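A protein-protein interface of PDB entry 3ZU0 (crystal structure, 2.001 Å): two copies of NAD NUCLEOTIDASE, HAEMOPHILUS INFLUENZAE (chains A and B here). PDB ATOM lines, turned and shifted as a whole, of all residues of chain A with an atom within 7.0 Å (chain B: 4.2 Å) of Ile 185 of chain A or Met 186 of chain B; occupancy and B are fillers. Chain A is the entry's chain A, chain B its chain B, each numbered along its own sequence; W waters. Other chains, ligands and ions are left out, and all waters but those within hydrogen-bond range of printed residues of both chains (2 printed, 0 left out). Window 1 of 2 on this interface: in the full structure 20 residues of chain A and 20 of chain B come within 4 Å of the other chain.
NE2 of Gln 192 of chain A lies within hydrogen-bond range of O of Tyr 143 of chain B, 2.9 Å away.
Ile 185 of chain B touches Thr 182 of chain A (CD1 to OG1, 3.6 Å). CG of Gln 184 of chain A touches OH of Tyr 177 of chain B, at 3.6 Å. O of Ala 126 of chain B touches CD1 of Ile 185 of chain A, at 3.7 Å. CD1 of Ile 129 of chain B touches CD1 of Ile 185 of chain A (3.9 Å). OG1 of Thr 182 of chain B touches CD1 of Ile 185 of chain A, at 3.7 Å. Ile 185 of chain A touches Met 186 of chain B. SD of Met 186 of chain A touches CG2 of Ile 185 of chain B, at 3.5 Å. CB of Ala 189 of chain B touches SD of Met 186 of chain A (3.9 Å). Asn 188 of chain A touches Ile 129 of chain B (ND2 to CD1, 3.8 Å). SD of Met 186 of chain B touches CB of Ala 189 of chain A (3.96 Å).
Ile 185 of chain A touches just these residues of chain B: Ala 126 (3.7 Å), Ile 129 (3.9 Å), Tyr 177 (3.9 Å), Thr 182 (3.7 Å), Ile 185 (3.9 Å) and Met 186 (3.5 Å). Met 186 of chain B touches just these residues of chain A: Ile 185 and Ala 189. Of the printed residues of chain A, Thr 182 of chain B touches Ile 185. Of the printed residues of chain A, Tyr 177 of chain B touches Gln 184 and Ile 185. Ile 156 of chain A touches none of the printed residues of chain B. Asn 188 of chain B touches none of the printed residues of chain A. The nearest printed residue of chain B that does not touch Ile 185 of chain A is Ala 183 of chain B (6.4 Å).
Of the 14 printed residues of chain B, 8 touch a printed residue of chain A. Hydrophobic or aromatic side chains of chain B that line the printed part of chain A: Ile 129, Tyr 143, Tyr 177, Ile 185, Met 186 and Ala 189. Printed residues of chain A that touch a printed residue of chain B: Thr 182, Gln 184, Ile 185, Met 186, Asn 188, Ala 189 and Gln 192. Hydrophobic or aromatic side chains of chain A that line the printed part of chain B: Ile 185, Met 186 and Ala 189. Among the printed residues, 15 pairs touch across the chains. Among the printed residues, no Asp or Glu carboxylate lies within 4 Å of a Lys or Arg side-chain nitrogen of the other chain.
Thr 182 of chain A touches Ile 185 of chain B, and with the chains exchanged Ile 185 of chain A touches Thr 182 of chain B. Ile 185 of chain A touches its own counterpart, Ile 185 of chain B. Ile 185 of chain A touches Met 186 of chain B, and with the chains exchanged Met 186 of chain A touches Ile 185 of chain B. Met 186 of chain A touches Ala 189 of chain B, and with the chains exchanged Ala 189 of chain A touches Met 186 of chain B. Positions printed for both chains: 156, 182, 183, 184, 185, 186, 187, 188, 189 and 190.
Water W2 lies within hydrogen-bond range of the side-chain hydroxyl of Tyr 177 of chain B (2.6 Å) and the side-chain amide oxygen of Gln 184 of chain A (2.8 Å). Water W1 bridges O of Ala 126 of chain B (2.7 Å) and ND2 of Asn 188 of chain A (2.8 Å).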
ATOM      1  N   ILE A 156       1.266   2.515   2.394  1.00  0.00           N
ATOM      2  CA  ILE A 156       0.350   1.451   2.817  1.00  0.00           C
ATOM      3  C   ILE A 156      -1.080   1.869   2.465  1.00  0.00           C
ATOM      4  O   ILE A 156      -1.464   3.025   2.672  1.00  0.00           O
ATOM      5  CB  ILE A 156       0.415   1.264   4.361  1.00  0.00           C
ATOM      6  CG1 ILE A 156       1.837   0.893   4.808  1.00  0.00           C
ATOM      7  CG2 ILE A 156      -0.634   0.237   4.854  1.00  0.00           C
ATOM      8  CD1 ILE A 156       2.104   1.128   6.317  1.00  0.00           C
ATOM      9  N   ILE A 180      -7.103   0.117  12.779  1.00  0.00           N
ATOM     10  CA  ILE A 180      -6.002   0.522  13.642  1.00  0.00           C
ATOM     11  C   ILE A 180      -4.912  -0.537  13.736  1.00  0.00           C
ATOM     12  O   ILE A 180      -3.737  -0.228  13.580  1.00  0.00           O
ATOM     13  CB  ILE A 180      -6.493   0.923  15.048  1.00  0.00           C
ATOM     14  CG1 ILE A 180      -7.192   2.273  14.971  1.00  0.00           C
ATOM     15  CG2 ILE A 180      -5.313   0.993  16.021  1.00  0.00           C
ATOM     16  CD1 ILE A 180      -7.994   2.636  16.180  1.00  0.00           C
ATOM     17  N   ALA A 181      -5.299  -1.788  13.964  1.00  0.00           N
ATOM     18  CA  ALA A 181      -4.332  -2.877  14.095  1.00  0.00           C
ATOM     19  C   ALA A 181      -3.511  -3.042  12.814  1.00  0.00           C
ATOM     20  O   ALA A 181      -2.280  -3.171  12.851  1.00  0.00           O
ATOM     21  CB  ALA A 181      -5.044  -4.179  14.439  1.00  0.00           C
ATOM     22  N   THR A 182      -4.196  -3.031  11.677  1.00  0.00           N
ATOM     23  CA  THR A 182      -3.518  -3.171  10.400  1.00  0.00           C
ATOM     24  C   THR A 182      -2.495  -2.064  10.207  1.00  0.00           C
ATOM     25  O   THR A 182      -1.384  -2.320   9.745  1.00  0.00           O
ATOM     26  CB  THR A 182      -4.509  -3.167   9.235  1.00  0.00           C
ATOM     27  OG1 THR A 182      -5.398  -4.289   9.365  1.00  0.00           O
ATOM     28  CG2 THR A 182      -3.772  -3.276   7.913  1.00  0.00           C
ATOM     29  N   ALA A 183      -2.861  -0.831  10.561  1.00  0.00           N
ATOM     30  CA  ALA A 183      -1.950   0.288  10.368  1.00  0.00           C
ATOM     31  C   ALA A 183      -0.685   0.089  11.200  1.00  0.00           C
ATOM     32  O   ALA A 183       0.407   0.309  10.715  1.00  0.00           O
ATOM     33  CB  ALA A 183      -2.619   1.615  10.720  1.00  0.00           C
ATOM     34  N   GLN A 184      -0.830  -0.343  12.447  1.00  0.00           N
ATOM     35  CA  GLN A 184       0.339  -0.507  13.296  1.00  0.00           C
ATOM     36  C   GLN A 184       1.185  -1.728  12.937  1.00  0.00           C
ATOM     37  O   GLN A 184       2.419  -1.661  12.958  1.00  0.00           O
ATOM     38  CB  GLN A 184      -0.053  -0.586  14.769  1.00  0.00           C
ATOM     39  CG  GLN A 184       1.169  -0.650  15.713  1.00  0.00           C
ATOM     40  CD  GLN A 184       2.071   0.585  15.619  1.00  0.00           C
ATOM     41  OE1 GLN A 184       1.951   1.504  16.415  1.00  0.00           O
ATOM     42  NE2 GLN A 184       2.979   0.600  14.644  1.00  0.00           N
ATOM     43  N   ILE A 185       0.529  -2.845  12.634  1.00  0.00           N
ATOM     44  CA  ILE A 185       1.253  -4.070  12.297  1.00  0.00           C
ATOM     45  C   ILE A 185       2.041  -3.862  11.010  1.00  0.00           C
ATOM     46  O   ILE A 185       3.222  -4.208  10.940  1.00  0.00           O
ATOM     47  CB  ILE A 185       0.318  -5.285  12.127  1.00  0.00           C
ATOM     48  CG1 ILE A 185      -0.417  -5.586  13.435  1.00  0.00           C
ATOM     49  CG2 ILE A 185       1.101  -6.487  11.672  1.00  0.00           C
ATOM     50  CD1 ILE A 185       0.473  -5.507  14.665  1.00  0.00           C
ATOM     51  N   MET A 186       1.395  -3.279   9.999  1.00  0.00           N
ATOM     52  CA  MET A 186       2.085  -2.951   8.756  1.00  0.00           C
ATOM     53  C   MET A 186       3.282  -2.050   8.996  1.00  0.00           C
ATOM     54  O   MET A 186       4.371  -2.306   8.496  1.00  0.00           O
ATOM     55  CB  MET A 186       1.142  -2.263   7.748  1.00  0.00           C
ATOM     56  CG  MET A 186       0.061  -3.168   7.194  1.00  0.00           C
ATOM     57  SD  MET A 186       0.827  -4.668   6.224  1.00  0.00           S
ATOM     58  CE  MET A 186       1.892  -3.688   4.970  1.00  0.00           C
ATOM     59  N   ALA A 187       3.064  -0.961   9.712  1.00  0.00           N
ATOM     60  CA  ALA A 187       4.130   0.019   9.919  1.00  0.00           C
ATOM     61  C   ALA A 187       5.283  -0.599  10.726  1.00  0.00           C
ATOM     62  O   ALA A 187       6.449  -0.426  10.391  1.00  0.00           O
ATOM     63  CB  ALA A 187       3.589   1.257  10.608  1.00  0.00           C
ATOM     64  N   ASN A 188       4.944  -1.341  11.771  1.00  0.00           N
ATOM     65  CA  ASN A 188       5.949  -2.023  12.599  1.00  0.00           C
ATOM     66  C   ASN A 188       6.819  -2.972  11.776  1.00  0.00           C
ATOM     67  O   ASN A 188       8.037  -2.946  11.901  1.00  0.00           O
ATOM     68  CB  ASN A 188       5.271  -2.787  13.743  1.00  0.00           C
ATOM     69  CG  ASN A 188       6.261  -3.312  14.774  1.00  0.00           C
ATOM     70  OD1 ASN A 188       7.061  -2.560  15.303  1.00  0.00           O
ATOM     71  ND2 ASN A 188       6.183  -4.605  15.074  1.00  0.00           N
ATOM     72  N   ALA A 189       6.193  -3.793  10.930  1.00  0.00           N
ATOM     73  CA  ALA A 189       6.911  -4.731  10.074  1.00  0.00           C
ATOM     74  C   ALA A 189       7.886  -4.054   9.097  1.00  0.00           C
ATOM     75  O   ALA A 189       8.923  -4.620   8.738  1.00  0.00           O
ATOM     76  CB  ALA A 189       5.933  -5.579   9.292  1.00  0.00           C
ATOM     77  N   LEU A 190       7.541  -2.852   8.649  1.00  0.00           N
ATOM     78  CA  LEU A 190       8.326  -2.165   7.623  1.00  0.00           C
ATOM     79  C   LEU A 190       9.641  -1.607   8.174  1.00  0.00           C
ATOM     80  O   LEU A 190      10.606  -1.388   7.429  1.00  0.00           O
ATOM     81  CB  LEU A 190       7.485  -1.066   6.970  1.00  0.00           C
ATOM     82  CG  LEU A 190       6.460  -1.626   5.968  1.00  0.00           C
ATOM     83  CD1 LEU A 190       5.379  -0.609   5.559  1.00  0.00           C
ATOM     84  CD2 LEU A 190       7.179  -2.148   4.737  1.00  0.00           C
ATOM     85  N   GLN A 192      12.128  -2.892   9.989  1.00  0.00           N
ATOM     86  CA  GLN A 192      13.362  -3.669   9.854  1.00  0.00           C
ATOM     87  C   GLN A 192      13.858  -3.777   8.414  1.00  0.00           C
ATOM     88  O   GLN A 192      14.963  -4.282   8.175  1.00  0.00           O
ATOM     89  CB  GLN A 192      13.208  -5.065  10.457  1.00  0.00           C
ATOM     90  CG  GLN A 192      12.225  -5.971   9.726  1.00  0.00           C
ATOM     91  CD  GLN A 192      11.866  -7.184  10.571  1.00  0.00           C
ATOM     92  OE1 GLN A 192      11.196  -7.058  11.589  1.00  0.00           O
ATOM     93  NE2 GLN A 192      12.331  -8.352  10.164  1.00  0.00           N
ATOM     94  N   VAL A 216      -1.180   5.280  16.872  1.00  0.00           N
ATOM     95  CA  VAL A 216      -0.277   4.392  16.159  1.00  0.00           C
ATOM     96  C   VAL A 216       1.050   5.120  15.881  1.00  0.00           C
ATOM     97  O   VAL A 216       1.054   6.307  15.534  1.00  0.00           O
ATOM     98  CB  VAL A 216      -0.909   3.900  14.807  1.00  0.00           C
ATOM     99  CG1 VAL A 216       0.105   3.120  13.960  1.00  0.00           C
ATOM    100  CG2 VAL A 216      -2.163   3.054  15.053  1.00  0.00           C
ATOM    101  N   ALA B 126       5.276 -10.324  17.000  1.00  0.00           N
ATOM    102  CA  ALA B 126       4.718  -9.352  16.052  1.00  0.00           C
ATOM    103  C   ALA B 126       3.581  -8.536  16.635  1.00  0.00           C
ATOM    104  O   ALA B 126       3.297  -7.445  16.144  1.00  0.00           O
ATOM    105  CB  ALA B 126       4.262 -10.042  14.759  1.00  0.00           C
ATOM    106  N   ILE B 129       4.246  -4.661  20.970  1.00  0.00           N
ATOM    107  CA  ILE B 129       5.010  -3.585  20.347  1.00  0.00           C
ATOM    108  C   ILE B 129       5.291  -2.457  21.337  1.00  0.00           C
ATOM    109  O   ILE B 129       4.392  -1.734  21.719  1.00  0.00           O
ATOM    110  CB  ILE B 129       4.226  -3.006  19.142  1.00  0.00           C
ATOM    111  CG1 ILE B 129       3.821  -4.136  18.185  1.00  0.00           C
ATOM    112  CG2 ILE B 129       5.039  -1.916  18.423  1.00  0.00           C
ATOM    113  CD1 ILE B 129       3.067  -3.678  16.948  1.00  0.00           C
ATOM    114  N   TYR B 143       9.345 -10.399  12.947  1.00  0.00           N
ATOM    115  CA  TYR B 143       9.550 -11.547  12.073  1.00  0.00           C
ATOM    116  C   TYR B 143      11.006 -11.620  11.643  1.00  0.00           C
ATOM    117  O   TYR B 143      11.761 -10.673  11.845  1.00  0.00           O
ATOM    118  CB  TYR B 143       8.649 -11.466  10.836  1.00  0.00           C
ATOM    119  CG  TYR B 143       9.093 -10.455   9.791  1.00  0.00           C
ATOM    120  CD1 TYR B 143       8.751  -9.116   9.902  1.00  0.00           C
ATOM    121  CD2 TYR B 143       9.829 -10.858   8.670  1.00  0.00           C
ATOM    122  CE1 TYR B 143       9.152  -8.185   8.923  1.00  0.00           C
ATOM    123  CE2 TYR B 143      10.228  -9.947   7.701  1.00  0.00           C
ATOM    124  CZ  TYR B 143       9.896  -8.620   7.840  1.00  0.00           C
ATOM    125  OH  TYR B 143      10.297  -7.735   6.882  1.00  0.00           O
ATOM    126  N   ILE B 156       7.349 -15.754  11.957  1.00  0.00           N
ATOM    127  CA  ILE B 156       6.635 -14.689  12.639  1.00  0.00           C
ATOM    128  C   ILE B 156       6.415 -15.069  14.108  1.00  0.00           C
ATOM    129  O   ILE B 156       5.987 -16.180  14.406  1.00  0.00           O
ATOM    130  CB  ILE B 156       5.237 -14.505  11.987  1.00  0.00           C
ATOM    131  CG1 ILE B 156       5.362 -14.121  10.490  1.00  0.00           C
ATOM    132  CG2 ILE B 156       4.415 -13.461  12.734  1.00  0.00           C
ATOM    133  CD1 ILE B 156       4.063 -14.336   9.705  1.00  0.00           C
ATOM    134  N   TYR B 177      -1.623  -6.344  20.150  1.00  0.00           N
ATOM    135  CA  TYR B 177      -2.571  -6.393  19.029  1.00  0.00           C
ATOM    136  C   TYR B 177      -3.222  -7.769  18.852  1.00  0.00           C
ATOM    137  O   TYR B 177      -2.685  -8.782  19.306  1.00  0.00           O
ATOM    138  CB  TYR B 177      -1.908  -5.848  17.750  1.00  0.00           C
ATOM    139  CG  TYR B 177      -1.588  -4.390  17.955  1.00  0.00           C
ATOM    140  CD1 TYR B 177      -0.392  -4.011  18.552  1.00  0.00           C
ATOM    141  CD2 TYR B 177      -2.518  -3.398  17.641  1.00  0.00           C
ATOM    142  CE1 TYR B 177      -0.107  -2.686  18.813  1.00  0.00           C
ATOM    143  CE2 TYR B 177      -2.246  -2.062  17.886  1.00  0.00           C
ATOM    144  CZ  TYR B 177      -1.029  -1.716  18.478  1.00  0.00           C
ATOM    145  OH  TYR B 177      -0.709  -0.409  18.730  1.00  0.00           O
ATOM    146  N   THR B 182      -3.175  -9.868  13.492  1.00  0.00           N
ATOM    147  CA  THR B 182      -1.728  -9.785  13.343  1.00  0.00           C
ATOM    148  C   THR B 182      -1.162 -10.909  12.485  1.00  0.00           C
ATOM    149  O   THR B 182      -0.315 -10.674  11.633  1.00  0.00           O
ATOM    150  CB  THR B 182      -1.013  -9.785  14.710  1.00  0.00           C
ATOM    151  OG1 THR B 182      -1.416  -8.621  15.458  1.00  0.00           O
ATOM    152  CG2 THR B 182       0.496  -9.746  14.501  1.00  0.00           C
ATOM    153  N   ALA B 183      -1.642 -12.137  12.688  1.00  0.00           N
ATOM    154  CA  ALA B 183      -1.119 -13.259  11.919  1.00  0.00           C
ATOM    155  C   ALA B 183      -1.403 -13.094  10.410  1.00  0.00           C
ATOM    156  O   ALA B 183      -0.506 -13.233   9.586  1.00  0.00           O
ATOM    157  CB  ALA B 183      -1.683 -14.582  12.443  1.00  0.00           C
ATOM    158  N   GLN B 184      -2.649 -12.781  10.059  1.00  0.00           N
ATOM    159  CA  GLN B 184      -3.019 -12.601   8.653  1.00  0.00           C
ATOM    160  C   GLN B 184      -2.289 -11.421   8.017  1.00  0.00           C
ATOM    161  O   GLN B 184      -1.762 -11.537   6.903  1.00  0.00           O
ATOM    162  CB  GLN B 184      -4.525 -12.402   8.495  1.00  0.00           C
ATOM    163  CG  GLN B 184      -4.998 -12.378   7.006  1.00  0.00           C
ATOM    164  CD  GLN B 184      -4.631 -13.634   6.215  1.00  0.00           C
ATOM    165  OE1 GLN B 184      -5.417 -14.562   6.125  1.00  0.00           O
ATOM    166  NE2 GLN B 184      -3.447 -13.656   5.632  1.00  0.00           N
ATOM    167  N   ILE B 185      -2.248 -10.294   8.718  1.00  0.00           N
ATOM    168  CA  ILE B 185      -1.631  -9.084   8.147  1.00  0.00           C
ATOM    169  C   ILE B 185      -0.129  -9.287   7.904  1.00  0.00           C
ATOM    170  O   ILE B 185       0.383  -8.944   6.836  1.00  0.00           O
ATOM    171  CB  ILE B 185      -1.841  -7.849   9.041  1.00  0.00           C
ATOM    172  CG1 ILE B 185      -3.326  -7.515   9.154  1.00  0.00           C
ATOM    173  CG2 ILE B 185      -1.060  -6.654   8.480  1.00  0.00           C
ATOM    174  CD1 ILE B 185      -3.969  -7.234   7.824  1.00  0.00           C
ATOM    175  N   MET B 186       0.570  -9.835   8.901  1.00  0.00           N
ATOM    176  CA  MET B 186       1.975 -10.222   8.739  1.00  0.00           C
ATOM    177  C   MET B 186       2.200 -11.186   7.566  1.00  0.00           C
ATOM    178  O   MET B 186       3.035 -10.926   6.701  1.00  0.00           O
ATOM    179  CB  MET B 186       2.510 -10.872  10.011  1.00  0.00           C
ATOM    180  CG  MET B 186       2.626  -9.963  11.220  1.00  0.00           C
ATOM    181  SD  MET B 186       3.863  -8.528  10.924  1.00  0.00           S
ATOM    182  CE  MET B 186       5.364  -9.532  10.221  1.00  0.00           C
ATOM    183  N   ALA B 187       1.479 -12.310   7.548  1.00  0.00           N
ATOM    184  CA  ALA B 187       1.631 -13.267   6.443  1.00  0.00           C
ATOM    185  C   ALA B 187       1.294 -12.639   5.072  1.00  0.00           C
ATOM    186  O   ALA B 187       1.964 -12.907   4.074  1.00  0.00           O
ATOM    187  CB  ALA B 187       0.795 -14.531   6.676  1.00  0.00           C
ATOM    188  N   ASN B 188       0.251 -11.816   5.035  1.00  0.00           N
ATOM    189  CA  ASN B 188      -0.144 -11.157   3.796  1.00  0.00           C
ATOM    190  C   ASN B 188       0.971 -10.260   3.263  1.00  0.00           C
ATOM    191  O   ASN B 188       1.265 -10.259   2.062  1.00  0.00           O
ATOM    192  CB  ASN B 188      -1.411 -10.335   3.998  1.00  0.00           C
ATOM    193  CG  ASN B 188      -1.989  -9.834   2.691  1.00  0.00           C
ATOM    194  OD1 ASN B 188      -2.214 -10.611   1.770  1.00  0.00           O
ATOM    195  ND2 ASN B 188      -2.218  -8.528   2.602  1.00  0.00           N
ATOM    196  N   ALA B 189       1.610  -9.522   4.165  1.00  0.00           N
ATOM    197  CA  ALA B 189       2.679  -8.602   3.782  1.00  0.00           C
ATOM    198  C   ALA B 189       3.937  -9.314   3.287  1.00  0.00           C
ATOM    199  O   ALA B 189       4.665  -8.783   2.449  1.00  0.00           O
ATOM    200  CB  ALA B 189       3.012  -7.664   4.923  1.00  0.00           C
ATOM    201  N   LEU B 190       4.195 -10.514   3.794  1.00  0.00           N
ATOM    202  CA  LEU B 190       5.412 -11.243   3.421  1.00  0.00           C
ATOM    203  C   LEU B 190       5.373 -11.830   2.018  1.00  0.00           C
ATOM    204  O   LEU B 190       6.427 -12.071   1.424  1.00  0.00           O
ATOM    205  CB  LEU B 190       5.731 -12.340   4.434  1.00  0.00           C
ATOM    206  CG  LEU B 190       6.292 -11.760   5.730  1.00  0.00           C
ATOM    207  CD1 LEU B 190       6.217 -12.765   6.882  1.00  0.00           C
ATOM    208  CD2 LEU B 190       7.731 -11.300   5.502  1.00  0.00           C
HETATM  209  O   HOH W   1       4.163  -6.221  13.944  1.00  0.00           O
HETATM  210  O   HOH W   2       1.614   0.757  19.128  1.00  0.00           O
